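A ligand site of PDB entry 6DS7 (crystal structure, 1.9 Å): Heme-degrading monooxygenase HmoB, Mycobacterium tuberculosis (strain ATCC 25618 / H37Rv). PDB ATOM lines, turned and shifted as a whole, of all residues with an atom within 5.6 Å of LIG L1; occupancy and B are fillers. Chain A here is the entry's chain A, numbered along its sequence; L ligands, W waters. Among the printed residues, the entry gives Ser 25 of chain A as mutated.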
ATOM      1  N   LYS A  20      26.750  18.628  21.854  1.00  0.00           N
ATOM      2  CA  LYS A  20      27.820  18.840  20.871  1.00  0.00           C
ATOM      3  C   LYS A  20      28.371  17.511  20.330  1.00  0.00           C
ATOM      4  O   LYS A  20      28.712  17.410  19.145  1.00  0.00           O
ATOM      5  CB  LYS A  20      28.950  19.654  21.509  1.00  0.00           C
ATOM      6  CG  LYS A  20      30.186  19.774  20.583  1.00  0.00           C
ATOM      7  CD  LYS A  20      31.566  19.777  21.290  1.00  0.00           C
ATOM      8  CE  LYS A  20      31.708  18.655  22.287  1.00  0.00           C
ATOM      9  NZ  LYS A  20      33.037  18.042  22.290  1.00  0.00           N
ATOM     10  N   ARG A  21      28.492  16.481  21.175  1.00  0.00           N
ATOM     11  CA  ARG A  21      28.984  15.179  20.719  1.00  0.00           C
ATOM     12  C   ARG A  21      28.067  14.532  19.697  1.00  0.00           C
ATOM     13  O   ARG A  21      28.494  13.664  18.935  1.00  0.00           O
ATOM     14  CB  ARG A  21      29.223  14.243  21.919  1.00  0.00           C
ATOM     15  CG  ARG A  21      30.413  14.717  22.750  1.00  0.00           C
ATOM     16  CD  ARG A  21      30.583  13.942  24.075  1.00  0.00           C
ATOM     17  NE  ARG A  21      31.683  14.503  24.865  1.00  0.00           N
ATOM     18  CZ  ARG A  21      32.462  13.803  25.681  1.00  0.00           C
ATOM     19  NH1 ARG A  21      32.268  12.491  25.824  1.00  0.00           N
ATOM     20  NH2 ARG A  21      33.437  14.409  26.337  1.00  0.00           N
ATOM     21  N   HIS A  24      27.664  16.125  14.857  1.00  0.00           N
ATOM     22  CA  HIS A  24      28.043  15.594  13.548  1.00  0.00           C
ATOM     23  C   HIS A  24      27.863  14.083  13.413  1.00  0.00           C
ATOM     24  O   HIS A  24      28.582  13.445  12.654  1.00  0.00           O
ATOM     25  CB  HIS A  24      29.451  16.067  13.188  1.00  0.00           C
ATOM     26  CG  HIS A  24      29.461  17.486  12.744  1.00  0.00           C
ATOM     27  ND1 HIS A  24      29.570  18.545  13.626  1.00  0.00           N
ATOM     28  CD2 HIS A  24      29.258  18.039  11.518  1.00  0.00           C
ATOM     29  CE1 HIS A  24      29.494  19.680  12.960  1.00  0.00           C
ATOM     30  NE2 HIS A  24      29.303  19.397  11.685  1.00  0.00           N
ATOM     31  N   SER A  25      26.946  13.487  14.172  1.00  0.00           N
ATOM     32  CA  SER A  25      26.880  12.045  14.258  1.00  0.00           C
ATOM     33  C   SER A  25      25.998  11.418  13.162  1.00  0.00           C
ATOM     34  O   SER A  25      26.005  10.176  13.004  1.00  0.00           O
ATOM     35  CB  SER A  25      26.322  11.655  15.648  1.00  0.00           C
ATOM     36  OG  SER A  25      24.974  12.129  15.784  1.00  0.00           O
ATOM     37  N   HIS A  27      26.172  10.910  10.008  1.00  0.00           N
ATOM     38  CA  HIS A  27      26.825   9.984   9.088  1.00  0.00           C
ATOM     39  C   HIS A  27      26.956   8.601   9.681  1.00  0.00           C
ATOM     40  O   HIS A  27      27.030   7.606   8.939  1.00  0.00           O
ATOM     41  CB  HIS A  27      28.223  10.503   8.694  1.00  0.00           C
ATOM     42  CG  HIS A  27      29.254  10.328   9.770  1.00  0.00           C
ATOM     43  ND1 HIS A  27      29.473  11.266  10.762  1.00  0.00           N
ATOM     44  CD2 HIS A  27      30.108   9.302  10.035  1.00  0.00           C
ATOM     45  CE1 HIS A  27      30.422  10.839  11.576  1.00  0.00           C
ATOM     46  NE2 HIS A  27      30.822   9.648  11.163  1.00  0.00           N
ATOM     47  N   ALA A  28      26.996   8.496  11.013  1.00  0.00           N
ATOM     48  CA  ALA A  28      27.281   7.186  11.567  1.00  0.00           C
ATOM     49  C   ALA A  28      26.104   6.239  11.444  1.00  0.00           C
ATOM     50  O   ALA A  28      26.289   5.031  11.656  1.00  0.00           O
ATOM     51  CB  ALA A  28      27.695   7.301  13.022  1.00  0.00           C
ATOM     52  N   PHE A  62      18.398  -2.907  13.632  1.00  0.00           N
ATOM     53  CA  PHE A  62      19.093  -2.194  14.711  1.00  0.00           C
ATOM     54  C   PHE A  62      20.327  -2.964  15.179  1.00  0.00           C
ATOM     55  O   PHE A  62      21.403  -2.373  15.354  1.00  0.00           O
ATOM     56  CB  PHE A  62      18.145  -1.948  15.884  1.00  0.00           C
ATOM     57  CG  PHE A  62      18.853  -1.657  17.144  1.00  0.00           C
ATOM     58  CD1 PHE A  62      19.485  -0.430  17.315  1.00  0.00           C
ATOM     59  CD2 PHE A  62      18.958  -2.620  18.155  1.00  0.00           C
ATOM     60  CE1 PHE A  62      20.188  -0.155  18.493  1.00  0.00           C
ATOM     61  CE2 PHE A  62      19.653  -2.343  19.344  1.00  0.00           C
ATOM     62  CZ  PHE A  62      20.265  -1.108  19.515  1.00  0.00           C
ATOM     63  N   TRP A  65      23.291  -2.750  12.872  1.00  0.00           N
ATOM     64  CA  TRP A  65      23.997  -1.489  13.020  1.00  0.00           C
ATOM     65  C   TRP A  65      24.770  -1.451  14.326  1.00  0.00           C
ATOM     66  O   TRP A  65      25.921  -0.992  14.358  1.00  0.00           O
ATOM     67  CB  TRP A  65      23.033  -0.291  12.973  1.00  0.00           C
ATOM     68  CG  TRP A  65      23.727   1.049  13.224  1.00  0.00           C
ATOM     69  CD1 TRP A  65      24.506   1.729  12.352  1.00  0.00           C
ATOM     70  CD2 TRP A  65      23.622   1.886  14.399  1.00  0.00           C
ATOM     71  NE1 TRP A  65      24.936   2.921  12.915  1.00  0.00           N
ATOM     72  CE2 TRP A  65      24.399   3.039  14.170  1.00  0.00           C
ATOM     73  CE3 TRP A  65      22.961   1.758  15.622  1.00  0.00           C
ATOM     74  CZ2 TRP A  65      24.536   4.069  15.125  1.00  0.00           C
ATOM     75  CZ3 TRP A  65      23.103   2.788  16.590  1.00  0.00           C
ATOM     76  CH2 TRP A  65      23.903   3.918  16.329  1.00  0.00           C
ATOM     77  N   ALA A  66      24.134  -1.891  15.420  1.00  0.00           N
ATOM     78  CA  ALA A  66      24.783  -1.769  16.721  1.00  0.00           C
ATOM     79  C   ALA A  66      26.088  -2.557  16.758  1.00  0.00           C
ATOM     80  O   ALA A  66      27.094  -2.064  17.297  1.00  0.00           O
ATOM     81  CB  ALA A  66      23.867  -2.269  17.843  1.00  0.00           C
ATOM     82  N   ALA A  70      28.100   0.905  14.105  1.00  0.00           N
ATOM     83  CA  ALA A  70      28.169   1.723  15.310  1.00  0.00           C
ATOM     84  C   ALA A  70      29.545   1.619  15.989  1.00  0.00           C
ATOM     85  O   ALA A  70      30.158   2.636  16.374  1.00  0.00           O
ATOM     86  CB  ALA A  70      27.039   1.320  16.273  1.00  0.00           C
ATOM     87  N   ALA A  73      32.197   3.416  14.026  1.00  0.00           N
ATOM     88  CA  ALA A  73      32.166   4.885  14.039  1.00  0.00           C
ATOM     89  C   ALA A  73      32.971   5.481  15.182  1.00  0.00           C
ATOM     90  O   ALA A  73      33.164   6.706  15.199  1.00  0.00           O
ATOM     91  CB  ALA A  73      30.729   5.412  14.149  1.00  0.00           C
ATOM     92  N   HIS A  74      33.440   4.681  16.137  1.00  0.00           N
ATOM     93  CA  HIS A  74      34.253   5.185  17.240  1.00  0.00           C
ATOM     94  C   HIS A  74      35.733   5.333  16.908  1.00  0.00           C
ATOM     95  O   HIS A  74      36.468   5.872  17.752  1.00  0.00           O
ATOM     96  CB  HIS A  74      34.139   4.269  18.451  1.00  0.00           C
ATOM     97  CG  HIS A  74      32.789   4.239  19.071  1.00  0.00           C
ATOM     98  ND1 HIS A  74      31.739   3.536  18.529  1.00  0.00           N
ATOM     99  CD2 HIS A  74      32.330   4.795  20.222  1.00  0.00           C
ATOM    100  CE1 HIS A  74      30.679   3.677  19.307  1.00  0.00           C
ATOM    101  NE2 HIS A  74      31.023   4.418  20.342  1.00  0.00           N
ATOM    102  N   HIS A  77      37.990   8.346  18.036  1.00  0.00           N
ATOM    103  CA  HIS A  77      37.310   9.048  19.113  1.00  0.00           C
ATOM    104  C   HIS A  77      37.745   8.570  20.498  1.00  0.00           C
ATOM    105  O   HIS A  77      37.957   7.365  20.730  1.00  0.00           O
ATOM    106  CB  HIS A  77      35.799   8.876  18.963  1.00  0.00           C
ATOM    107  CG  HIS A  77      35.249   9.517  17.729  1.00  0.00           C
ATOM    108  ND1 HIS A  77      34.555  10.714  17.757  1.00  0.00           N
ATOM    109  CD2 HIS A  77      35.307   9.135  16.431  1.00  0.00           C
ATOM    110  CE1 HIS A  77      34.191  11.034  16.521  1.00  0.00           C
ATOM    111  NE2 HIS A  77      34.632  10.100  15.701  1.00  0.00           N
ATOM    112  N   ARG A  78      37.904   9.518  21.422  1.00  0.00           N
ATOM    113  CA  ARG A  78      38.008   9.187  22.837  1.00  0.00           C
ATOM    114  C   ARG A  78      36.784   8.366  23.226  1.00  0.00           C
ATOM    115  O   ARG A  78      35.678   8.556  22.697  1.00  0.00           O
ATOM    116  CB  ARG A  78      38.053  10.469  23.682  1.00  0.00           C
ATOM    117  N   ALA A  79      36.971   7.405  24.127  1.00  0.00           N
ATOM    118  CA  ALA A  79      35.820   6.688  24.653  1.00  0.00           C
ATOM    119  C   ALA A  79      35.429   7.175  26.051  1.00  0.00           C
ATOM    120  O   ALA A  79      34.828   6.419  26.815  1.00  0.00           O
ATOM    121  CB  ALA A  79      36.064   5.179  24.632  1.00  0.00           C
ATOM    122  N   ASN A  80      35.779   8.440  26.402  1.00  0.00           N
ATOM    123  CA  ASN A  80      35.444   9.118  27.654  1.00  0.00           C
ATOM    124  C   ASN A  80      34.063   9.790  27.626  1.00  0.00           C
ATOM    125  O   ASN A  80      33.936  10.952  27.223  1.00  0.00           O
ATOM    126  CB  ASN A  80      36.528  10.141  27.989  1.00  0.00           C
ATOM    127  CG  ASN A  80      36.449  10.624  29.424  1.00  0.00           C
ATOM    128  OD1 ASN A  80      35.798  10.017  30.275  1.00  0.00           O
ATOM    129  ND2 ASN A  80      37.116  11.747  29.696  1.00  0.00           N
ATOM    130  N   PRO A  81      33.024   9.108  28.069  1.00  0.00           N
ATOM    131  CA  PRO A  81      31.673   9.672  27.984  1.00  0.00           C
ATOM    132  C   PRO A  81      31.433  10.799  28.989  1.00  0.00           C
ATOM    133  O   PRO A  81      32.043  10.857  30.054  1.00  0.00           O
ATOM    134  CB  PRO A  81      30.768   8.481  28.302  1.00  0.00           C
ATOM    135  CG  PRO A  81      31.630   7.527  29.095  1.00  0.00           C
ATOM    136  CD  PRO A  81      33.097   7.912  28.934  1.00  0.00           C
ATOM    137  N   VAL A  82      30.542  11.712  28.626  1.00  0.00           N
ATOM    138  CA  VAL A  82      30.122  12.684  29.628  1.00  0.00           C
ATOM    139  C   VAL A  82      28.863  12.179  30.347  1.00  0.00           C
ATOM    140  O   VAL A  82      28.625  12.514  31.504  1.00  0.00           O
ATOM    141  CB  VAL A  82      29.943  14.064  28.962  1.00  0.00           C
ATOM    142  CG1 VAL A  82      28.961  13.964  27.832  1.00  0.00           C
ATOM    143  CG2 VAL A  82      29.530  15.129  29.961  1.00  0.00           C
HETATM  144  C1  LIG L   1      30.272   8.327  20.100  1.00  0.00           C
HETATM  145  C2  LIG L   1      31.431   6.160  24.333  1.00  0.00           C
HETATM  146  C3  LIG L   1      28.581   2.426  23.152  1.00  0.00           C
HETATM  147  C4  LIG L   1      26.996   4.774  19.231  1.00  0.00           C
HETATM  148  C5  LIG L   1      30.820   8.111  21.368  1.00  0.00           C
HETATM  149  C6  LIG L   1      31.656   9.005  22.161  1.00  0.00           C
HETATM  150  C7  LIG L   1      31.929   8.406  23.306  1.00  0.00           C
HETATM  151  C8  LIG L   1      31.315   7.089  23.312  1.00  0.00           C
HETATM  152  C9  LIG L   1      32.765   9.015  24.452  1.00  0.00           C
HETATM  153  C10 LIG L   1      32.099  10.467  21.856  1.00  0.00           C
HETATM  154  C11 LIG L   1      33.107  10.602  20.731  1.00  0.00           C
HETATM  155  C12 LIG L   1      33.506  12.077  20.672  1.00  0.00           C
HETATM  156  O1  LIG L   1      33.100  12.875  21.563  1.00  0.00           O
HETATM  157  O2  LIG L   1      34.256  12.469  19.730  1.00  0.00           O
HETATM  158  C13 LIG L   1      30.801   4.931  24.375  1.00  0.00           C
HETATM  159  C14 LIG L   1      30.936   3.900  25.412  1.00  0.00           C
HETATM  160  C15 LIG L   1      30.142   2.880  25.076  1.00  0.00           C
HETATM  161  C16 LIG L   1      29.488   3.219  23.818  1.00  0.00           C
HETATM  162  C17 LIG L   1      31.829   4.023  26.677  1.00  0.00           C
HETATM  163  C18 LIG L   1      29.925   1.542  25.815  1.00  0.00           C
HETATM  164  C19 LIG L   1      30.388   1.313  27.056  1.00  0.00           C
HETATM  165  C20 LIG L   1      27.857   2.799  22.051  1.00  0.00           C
HETATM  166  C21 LIG L   1      26.813   1.999  21.477  1.00  0.00           C
HETATM  167  C22 LIG L   1      26.327   2.665  20.416  1.00  0.00           C
HETATM  168  C23 LIG L   1      27.123   3.860  20.239  1.00  0.00           C
HETATM  169  C24 LIG L   1      26.338   0.658  22.105  1.00  0.00           C
HETATM  170  C25 LIG L   1      25.198   2.291  19.468  1.00  0.00           C
HETATM  171  C26 LIG L   1      24.621   1.092  19.481  1.00  0.00           C
HETATM  172  C27 LIG L   1      27.774   5.902  19.070  1.00  0.00           C
HETATM  173  C28 LIG L   1      27.826   6.796  17.914  1.00  0.00           C
HETATM  174  C29 LIG L   1      28.726   7.772  18.178  1.00  0.00           C
HETATM  175  C30 LIG L   1      29.293   7.532  19.485  1.00  0.00           C
HETATM  176  C31 LIG L   1      26.986   6.617  16.629  1.00  0.00           C
HETATM  177  C32 LIG L   1      29.117   8.968  17.303  1.00  0.00           C
HETATM  178  C33 LIG L   1      30.293   8.641  16.398  1.00  0.00           C
HETATM  179  C34 LIG L   1      30.743   9.865  15.636  1.00  0.00           C
HETATM  180  O3  LIG L   1      31.152   9.696  14.463  1.00  0.00           O
HETATM  181  O4  LIG L   1      30.704  11.015  16.157  1.00  0.00           O
HETATM  182  N1  LIG L   1      30.634   6.944  22.108  1.00  0.00           N
HETATM  183  N2  LIG L   1      29.873   4.490  23.424  1.00  0.00           N
HETATM  184  N3  LIG L   1      28.064   3.905  21.257  1.00  0.00           N
HETATM  185  N4  LIG L   1      28.690   6.384  19.995  1.00  0.00           N
HETATM  186 FE1  LIG L   1      29.443   5.387  21.600  1.00  0.00          FE
HETATM  187  C1  LG2 L   2      27.156   6.966  24.076  1.00  0.00           C
HETATM  188  C2  LG2 L   2      24.440   3.074  23.437  1.00  0.00           C
HETATM  189  C3  LG2 L   2      22.206   5.174  19.655  1.00  0.00           C
HETATM  190  C4  LG2 L   2      25.730   8.455  19.690  1.00  0.00           C
HETATM  191  C5  LG2 L   2      26.559   5.744  24.296  1.00  0.00           C
HETATM  192  C6  LG2 L   2      26.793   4.858  25.429  1.00  0.00           C
HETATM  193  C7  LG2 L   2      26.040   3.789  25.252  1.00  0.00           C
HETATM  194  C8  LG2 L   2      25.310   3.958  23.995  1.00  0.00           C
HETATM  195  C9  LG2 L   2      25.933   2.560  26.174  1.00  0.00           C
HETATM  196  C10 LG2 L   2      27.732   5.145  26.635  1.00  0.00           C
HETATM  197  C11 LG2 L   2      27.005   6.217  27.469  1.00  0.00           C
HETATM  198  C12 LG2 L   2      27.578   6.229  28.877  1.00  0.00           C
HETATM  199  O1  LG2 L   2      28.850   6.225  29.011  1.00  0.00           O
HETATM  200  O2  LG2 L   2      26.778   6.252  29.872  1.00  0.00           O
HETATM  201  C13 LG2 L   2      23.538   3.363  22.423  1.00  0.00           C
HETATM  202  C14 LG2 L   2      22.414   2.567  22.140  1.00  0.00           C
HETATM  203  C15 LG2 L   2      21.770   3.119  21.104  1.00  0.00           C
HETATM  204  C16 LG2 L   2      22.493   4.290  20.683  1.00  0.00           C
HETATM  205  C17 LG2 L   2      22.059   1.302  22.948  1.00  0.00           C
HETATM  206  C18 LG2 L   2      20.478   2.580  20.459  1.00  0.00           C
HETATM  207  C19 LG2 L   2      19.495   3.462  20.293  1.00  0.00           C
HETATM  208  C20 LG2 L   2      23.028   6.184  19.234  1.00  0.00           C
HETATM  209  C21 LG2 L   2      22.933   6.937  18.009  1.00  0.00           C
HETATM  210  C22 LG2 L   2      23.909   7.863  18.060  1.00  0.00           C
HETATM  211  C23 LG2 L   2      24.637   7.704  19.287  1.00  0.00           C
HETATM  212  C24 LG2 L   2      21.862   6.735  16.892  1.00  0.00           C
HETATM  213  C25 LG2 L   2      24.322   8.926  17.018  1.00  0.00           C
HETATM  214  C26 LG2 L   2      24.232   8.741  15.694  1.00  0.00           C
HETATM  215  C27 LG2 L   2      26.294   8.368  20.920  1.00  0.00           C
HETATM  216  C28 LG2 L   2      27.241   9.337  21.439  1.00  0.00           C
HETATM  217  C29 LG2 L   2      27.647   8.949  22.621  1.00  0.00           C
HETATM  218  C30 LG2 L   2      26.990   7.688  22.910  1.00  0.00           C
HETATM  219  C31 LG2 L   2      27.679  10.590  20.644  1.00  0.00           C
HETATM  220  C32 LG2 L   2      28.658   9.678  23.536  1.00  0.00           C
HETATM  221  C33 LG2 L   2      27.903  10.168  24.767  1.00  0.00           C
HETATM  222  C34 LG2 L   2      28.880  10.819  25.735  1.00  0.00           C
HETATM  223  O3  LG2 L   2      28.522  11.004  26.917  1.00  0.00           O
HETATM  224  O4  LG2 L   2      30.030  11.150  25.373  1.00  0.00           O
HETATM  225  N1  LG2 L   2      25.632   5.170  23.444  1.00  0.00           N
HETATM  226  N2  LG2 L   2      23.555   4.417  21.554  1.00  0.00           N
HETATM  227  N3  LG2 L   2      24.098   6.700  19.991  1.00  0.00           N
HETATM  228  N4  LG2 L   2      26.147   7.379  21.856  1.00  0.00           N
HETATM  229 FE1  LG2 L   2      24.634   6.113  21.785  1.00  0.00          FE
HETATM  230  O   HOH W   1      32.599  14.713  18.487  1.00  0.00           O
HETATM  231  O   HOH W   2      30.896  12.145  18.307  1.00  0.00           O
HETATM  232  O   HOH W   3      33.196  15.945  21.053  1.00  0.00           O
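A ring nitrogen (ND1) of His 74 sits at hydrogen-bond distance from the backbone carbonyl oxygen (O) of Ala 70, 2.8 Å away.
The guanidinium group (NH1) of Arg 21 sits at hydrogen-bond distance from the backbone carbonyl oxygen (O) of Asn 80.
N of Ala 70 is in hydrogen-bond range of O of Trp 65 (2.9 Å).
NE1 of Trp 65 lies within hydrogen-bond range of O of Ala 28.
ND1 of His 27 sits at hydrogen-bond distance from O of His 24, at 3.0 Å.
Water W2 bridges an oxygen (O4) of LIG L1 (2.4 Å) and the backbone carbonyl oxygen of Arg 21 (2.9 Å).
Water W3 bridges NZ of Lys 20 and O1 of LIG L1.
Residues that only touch LIG L1: Arg 78 (3.4 Å), Asn 80 (3.5 Å), Trp 65 (3.6 Å), Ala 79 (3.6 Å), Pro 81 (3.6 Å), Ala 73 (3.7 Å), Ala 28 (3.7 Å), Ala 70 (3.8 Å) and Ala 66 (3.8 Å).
Hydrophobic or aromatic side chains that line LIG L1: His 27, Ala 28, Trp 65, Ala 66, Ala 70, Ala 73, His 74 and His 77.
The nearest printed residue that does not touch LIG L1 is Ser 25 (4.2 Å).
An oxygen (O4) of LG2 L2 is in salt-bridge range of the guanidinium group (NH1) of Arg 21 (2.6 Å).
N of Val 82 lies within hydrogen-bond range of O3 of LG2 L2.
An oxygen (O1) of LIG L1 lies within salt-bridge range of the guanidinium group (NE) of Arg 21.
An oxygen (O2) of LIG L1 is in hydrogen-bond range of a ring nitrogen (ND1) of His 77 (2.7 Å).
A ring nitrogen (NE2) of His 27 sits close to an oxygen (O3) of LIG L1, at 3.3 Å.
A ring nitrogen (NE2) of His 74 is bound to an iron atom (FE1) of LIG L1 (2.2 Å).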
